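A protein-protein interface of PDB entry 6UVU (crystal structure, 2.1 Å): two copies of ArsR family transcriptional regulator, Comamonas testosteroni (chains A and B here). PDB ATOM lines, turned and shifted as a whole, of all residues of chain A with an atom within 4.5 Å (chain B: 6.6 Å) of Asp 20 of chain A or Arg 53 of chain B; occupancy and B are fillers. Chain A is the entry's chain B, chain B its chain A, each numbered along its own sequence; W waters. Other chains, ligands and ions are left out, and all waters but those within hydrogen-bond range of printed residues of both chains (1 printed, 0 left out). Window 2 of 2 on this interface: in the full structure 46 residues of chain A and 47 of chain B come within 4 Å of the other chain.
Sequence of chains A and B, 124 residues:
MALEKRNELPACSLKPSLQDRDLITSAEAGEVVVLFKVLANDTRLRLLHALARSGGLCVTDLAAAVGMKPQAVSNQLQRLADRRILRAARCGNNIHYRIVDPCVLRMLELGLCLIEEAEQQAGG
The guanidinium group (NE) of Arg 53 of chain B lies within hydrogen-bond range of the backbone carbonyl oxygen (O) of Arg 21 of chain A (3.0 Å).
O of Ala 50 of chain B sits at hydrogen-bond distance from OG of Ser 54 of chain B. O of Leu 14 of chain A sits close to OE1 of Gln 19 of chain A, at 3.0 Å.
Among the printed residues, merely in contact across the chains: Asp 22 of chain A with His 49 of chain B (3.4 Å), Leu 23 of chain A with Ala 50 of chain B (3.6 Å), Leu 14 of chain A with Ala 52 of chain B (3.6 Å), Asp 20 of chain A with Arg 53 of chain B (3.8 Å), Asp 22 of chain A with Arg 53 of chain B (3.8 Å), Leu 23 of chain A with His 49 of chain B (3.9 Å) and Leu 23 of chain A with Arg 53 of chain B (3.9 Å).
Printed residues of chain B within 4 Å of Leu 14 of chain A: Ala 52 (3.6 Å). Gln 19 of chain A touches none of the printed residues of chain B. Asp 20 of chain A touches just one residue of chain B: Arg 53. Of the printed residues of chain B, Arg 21 of chain A touches Arg 53 (3.0 Å). Of the printed residues of chain B, Asp 22 of chain A touches His 49 and Arg 53. Printed residues of chain A within 4 Å of His 49 of chain B: Asp 22 and Leu 23. Of the printed residues of chain A, Arg 53 of chain B touches Asp 20 (3.8 Å), Arg 21 (3.0 Å), Asp 22 (3.8 Å) and Leu 23 (3.9 Å). The nearest printed residue of chain B that does not touch Asp 20 of chain A is His 49 of chain B (6.9 Å).
Of the 7 printed residues of chain A, 5 touch a printed residue of chain B. Printed residues of chain A that touch a printed residue of chain B: Leu 14, Asp 20, Arg 21, Asp 22 and Leu 23. Printed residues of chain B that touch a printed residue of chain A: His 49, Ala 50, Ala 52 and Arg 53.
No position is printed for both chains. Of the 8 pairs that touch across the chains among the printed residues, none has its exchanged pair printed and touching as well.
Water W1 lies within hydrogen-bond range of O of Leu 18 of chain A (2.7 Å), NE2 of His 49 of chain B (2.8 Å), O of Arg 21 of chain A (2.8 Å) and NE of Arg 53 of chain B (3.5 Å).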
ATOM      1  N   LEU A  14       0.175 -10.667   4.637  1.00  0.00           N
ATOM      2  CA  LEU A  14      -0.655  -9.714   3.909  1.00  0.00           C
ATOM      3  C   LEU A  14       0.188  -8.927   2.899  1.00  0.00           C
ATOM      4  O   LEU A  14       1.340  -8.566   3.171  1.00  0.00           O
ATOM      5  CB  LEU A  14      -1.328  -8.770   4.910  1.00  0.00           C
ATOM      6  CG  LEU A  14      -2.400  -7.778   4.474  1.00  0.00           C
ATOM      7  CD1 LEU A  14      -3.620  -8.502   3.950  1.00  0.00           C
ATOM      8  CD2 LEU A  14      -2.769  -6.904   5.658  1.00  0.00           C
ATOM      9  N   LEU A  18      -1.422  -3.423   1.309  1.00  0.00           N
ATOM     10  CA  LEU A  18      -2.649  -3.493   2.094  1.00  0.00           C
ATOM     11  C   LEU A  18      -2.411  -3.458   3.601  1.00  0.00           C
ATOM     12  O   LEU A  18      -3.381  -3.327   4.358  1.00  0.00           O
ATOM     13  CB  LEU A  18      -3.427  -4.759   1.724  1.00  0.00           C
ATOM     14  CG  LEU A  18      -4.037  -4.788   0.322  1.00  0.00           C
ATOM     15  CD1 LEU A  18      -4.679  -6.138   0.061  1.00  0.00           C
ATOM     16  CD2 LEU A  18      -5.051  -3.643   0.118  1.00  0.00           C
ATOM     17  N   GLN A  19      -1.154  -3.555   4.053  1.00  0.00           N
ATOM     18  CA  GLN A  19      -0.784  -3.630   5.463  1.00  0.00           C
ATOM     19  C   GLN A  19      -0.953  -2.313   6.212  1.00  0.00           C
ATOM     20  O   GLN A  19      -0.715  -2.276   7.427  1.00  0.00           O
ATOM     21  CB  GLN A  19       0.668  -4.099   5.596  1.00  0.00           C
ATOM     22  CG  GLN A  19       0.816  -5.561   5.954  1.00  0.00           C
ATOM     23  CD  GLN A  19       2.264  -5.993   5.982  1.00  0.00           C
ATOM     24  OE1 GLN A  19       2.738  -6.700   5.082  1.00  0.00           O
ATOM     25  NE2 GLN A  19       2.988  -5.560   7.012  1.00  0.00           N
ATOM     26  N   ASP A  20      -1.333  -1.238   5.523  1.00  0.00           N
ATOM     27  CA  ASP A  20      -1.493   0.067   6.151  1.00  0.00           C
ATOM     28  C   ASP A  20      -2.923   0.400   6.524  1.00  0.00           C
ATOM     29  O   ASP A  20      -3.137   1.086   7.525  1.00  0.00           O
ATOM     30  CB  ASP A  20      -0.978   1.172   5.226  1.00  0.00           C
ATOM     31  CG  ASP A  20       0.521   1.339   5.304  1.00  0.00           C
ATOM     32  OD1 ASP A  20       1.180   0.650   6.122  1.00  0.00           O
ATOM     33  OD2 ASP A  20       1.028   2.189   4.550  1.00  0.00           O
ATOM     34  N   ARG A  21      -3.892  -0.043   5.726  1.00  0.00           N
ATOM     35  CA  ARG A  21      -5.292   0.212   6.025  1.00  0.00           C
ATOM     36  C   ARG A  21      -5.611  -0.167   7.470  1.00  0.00           C
ATOM     37  O   ARG A  21      -5.120  -1.173   7.994  1.00  0.00           O
ATOM     38  CB  ARG A  21      -6.171  -0.566   5.039  1.00  0.00           C
ATOM     39  CG  ARG A  21      -7.644  -0.585   5.371  1.00  0.00           C
ATOM     40  CD  ARG A  21      -8.480  -0.781   4.123  1.00  0.00           C
ATOM     41  NE  ARG A  21      -8.825   0.501   3.525  1.00  0.00           N
ATOM     42  CZ  ARG A  21      -9.848   1.255   3.918  1.00  0.00           C
ATOM     43  NH1 ARG A  21     -10.633   0.855   4.910  1.00  0.00           N
ATOM     44  NH2 ARG A  21     -10.085   2.412   3.322  1.00  0.00           N
ATOM     45  N   ASP A  22      -6.385   0.688   8.134  1.00  0.00           N
ATOM     46  CA  ASP A  22      -6.864   0.374   9.473  1.00  0.00           C
ATOM     47  C   ASP A  22      -7.763  -0.857   9.458  1.00  0.00           C
ATOM     48  O   ASP A  22      -8.391  -1.197   8.444  1.00  0.00           O
ATOM     49  CB  ASP A  22      -7.642   1.549  10.055  1.00  0.00           C
ATOM     50  CG  ASP A  22      -6.786   2.752  10.238  1.00  0.00           C
ATOM     51  OD1 ASP A  22      -5.721   2.613  10.885  1.00  0.00           O
ATOM     52  OD2 ASP A  22      -7.164   3.821   9.711  1.00  0.00           O
ATOM     53  N   LEU A  23      -7.830  -1.514  10.618  1.00  0.00           N
ATOM     54  CA  LEU A  23      -8.734  -2.630  10.826  1.00  0.00           C
ATOM     55  C   LEU A  23     -10.120  -2.325  10.265  1.00  0.00           C
ATOM     56  O   LEU A  23     -10.703  -1.271  10.537  1.00  0.00           O
ATOM     57  CB  LEU A  23      -8.817  -2.952  12.317  1.00  0.00           C
ATOM     58  CG  LEU A  23      -9.617  -4.209  12.648  1.00  0.00           C
ATOM     59  CD1 LEU A  23      -8.945  -5.437  12.045  1.00  0.00           C
ATOM     60  CD2 LEU A  23      -9.796  -4.346  14.167  1.00  0.00           C
ATOM     61  N   LEU B  48      -9.867 -12.116  11.173  1.00  0.00           N
ATOM     62  CA  LEU B  48      -8.903 -12.502  10.153  1.00  0.00           C
ATOM     63  C   LEU B  48      -8.098 -11.299   9.674  1.00  0.00           C
ATOM     64  O   LEU B  48      -6.888 -11.420   9.433  1.00  0.00           O
ATOM     65  CB  LEU B  48      -9.636 -13.173   8.986  1.00  0.00           C
ATOM     66  CG  LEU B  48     -10.090 -14.586   9.354  1.00  0.00           C
ATOM     67  CD1 LEU B  48     -11.094 -15.099   8.315  1.00  0.00           C
ATOM     68  CD2 LEU B  48      -8.876 -15.527   9.452  1.00  0.00           C
ATOM     69  N   HIS B  49      -8.750 -10.141   9.500  1.00  0.00           N
ATOM     70  CA  HIS B  49      -8.008  -8.930   9.156  1.00  0.00           C
ATOM     71  C   HIS B  49      -6.969  -8.596  10.230  1.00  0.00           C
ATOM     72  O   HIS B  49      -5.800  -8.343   9.915  1.00  0.00           O
ATOM     73  CB  HIS B  49      -8.963  -7.756   8.923  1.00  0.00           C
ATOM     74  CG  HIS B  49      -8.310  -6.562   8.286  1.00  0.00           C
ATOM     75  ND1 HIS B  49      -8.966  -5.363   8.096  1.00  0.00           N
ATOM     76  CD2 HIS B  49      -7.061  -6.386   7.790  1.00  0.00           C
ATOM     77  CE1 HIS B  49      -8.148  -4.503   7.510  1.00  0.00           C
ATOM     78  NE2 HIS B  49      -6.982  -5.095   7.327  1.00  0.00           N
ATOM     79  N   ALA B  50      -7.365  -8.614  11.509  1.00  0.00           N
ATOM     80  CA  ALA B  50      -6.408  -8.337  12.584  1.00  0.00           C
ATOM     81  C   ALA B  50      -5.234  -9.318  12.568  1.00  0.00           C
ATOM     82  O   ALA B  50      -4.073  -8.922  12.747  1.00  0.00           O
ATOM     83  CB  ALA B  50      -7.120  -8.387  13.942  1.00  0.00           C
ATOM     84  N   LEU B  51      -5.521 -10.606  12.379  1.00  0.00           N
ATOM     85  CA  LEU B  51      -4.473 -11.615  12.305  1.00  0.00           C
ATOM     86  C   LEU B  51      -3.540 -11.374  11.119  1.00  0.00           C
ATOM     87  O   LEU B  51      -2.346 -11.701  11.191  1.00  0.00           O
ATOM     88  CB  LEU B  51      -5.116 -12.997  12.207  1.00  0.00           C
ATOM     89  CG  LEU B  51      -5.088 -13.974  13.384  1.00  0.00           C
ATOM     90  CD1 LEU B  51      -4.392 -13.429  14.625  1.00  0.00           C
ATOM     91  CD2 LEU B  51      -6.474 -14.492  13.698  1.00  0.00           C
ATOM     92  N   ALA B  52      -4.067 -10.805  10.028  1.00  0.00           N
ATOM     93  CA  ALA B  52      -3.310 -10.658   8.795  1.00  0.00           C
ATOM     94  C   ALA B  52      -2.358  -9.474   8.864  1.00  0.00           C
ATOM     95  O   ALA B  52      -1.214  -9.581   8.415  1.00  0.00           O
ATOM     96  CB  ALA B  52      -4.271 -10.508   7.611  1.00  0.00           C
ATOM     97  N   ARG B  53      -2.822  -8.342   9.405  1.00  0.00           N
ATOM     98  CA  ARG B  53      -1.955  -7.182   9.612  1.00  0.00           C
ATOM     99  C   ARG B  53      -0.783  -7.523  10.519  1.00  0.00           C
ATOM    100  O   ARG B  53       0.374  -7.222  10.205  1.00  0.00           O
ATOM    101  CB  ARG B  53      -2.745  -6.034  10.241  1.00  0.00           C
ATOM    102  CG  ARG B  53      -3.795  -5.385   9.378  1.00  0.00           C
ATOM    103  CD  ARG B  53      -4.521  -4.324  10.219  1.00  0.00           C
ATOM    104  NE  ARG B  53      -3.975  -2.975  10.048  1.00  0.00           N
ATOM    105  CZ  ARG B  53      -3.948  -2.052  11.006  1.00  0.00           C
ATOM    106  NH1 ARG B  53      -4.400  -2.334  12.221  1.00  0.00           N
ATOM    107  NH2 ARG B  53      -3.449  -0.847  10.752  1.00  0.00           N
ATOM    108  N   SER B  54      -1.077  -8.110  11.676  1.00  0.00           N
ATOM    109  CA  SER B  54      -0.065  -8.383  12.680  1.00  0.00           C
ATOM    110  C   SER B  54       0.762  -9.605  12.345  1.00  0.00           C
ATOM    111  O   SER B  54       1.856  -9.764  12.894  1.00  0.00           O
ATOM    112  CB  SER B  54      -0.727  -8.582  14.041  1.00  0.00           C
ATOM    113  OG  SER B  54      -1.630  -9.674  13.979  1.00  0.00           O
ATOM    114  N   GLY B  55       0.270 -10.467  11.462  1.00  0.00           N
ATOM    115  CA  GLY B  55       0.962 -11.716  11.250  1.00  0.00           C
ATOM    116  C   GLY B  55       0.803 -12.708  12.375  1.00  0.00           C
ATOM    117  O   GLY B  55       1.497 -13.727  12.386  1.00  0.00           O
ATOM    118  N   GLY B  56      -0.108 -12.453  13.312  1.00  0.00           N
ATOM    119  CA  GLY B  56      -0.340 -13.373  14.402  1.00  0.00           C
ATOM    120  C   GLY B  56      -0.406 -12.687  15.750  1.00  0.00           C
ATOM    121  O   GLY B  56       0.430 -11.832  16.053  1.00  0.00           O
ATOM    122  N   LEU B 108      -9.573 -12.450   1.496  1.00  0.00           N
ATOM    123  CA  LEU B 108      -9.603 -11.266   2.351  1.00  0.00           C
ATOM    124  C   LEU B 108      -8.976 -10.069   1.657  1.00  0.00           C
ATOM    125  O   LEU B 108      -9.513  -8.957   1.710  1.00  0.00           O
ATOM    126  CB  LEU B 108      -8.868 -11.555   3.662  1.00  0.00           C
ATOM    127  CG  LEU B 108      -8.682 -10.418   4.676  1.00  0.00           C
ATOM    128  CD1 LEU B 108     -10.040 -10.000   5.277  1.00  0.00           C
ATOM    129  CD2 LEU B 108      -7.687 -10.798   5.808  1.00  0.00           C
HETATM  130  O   HOH W   1      -4.691  -3.651   6.728  1.00  0.00           O
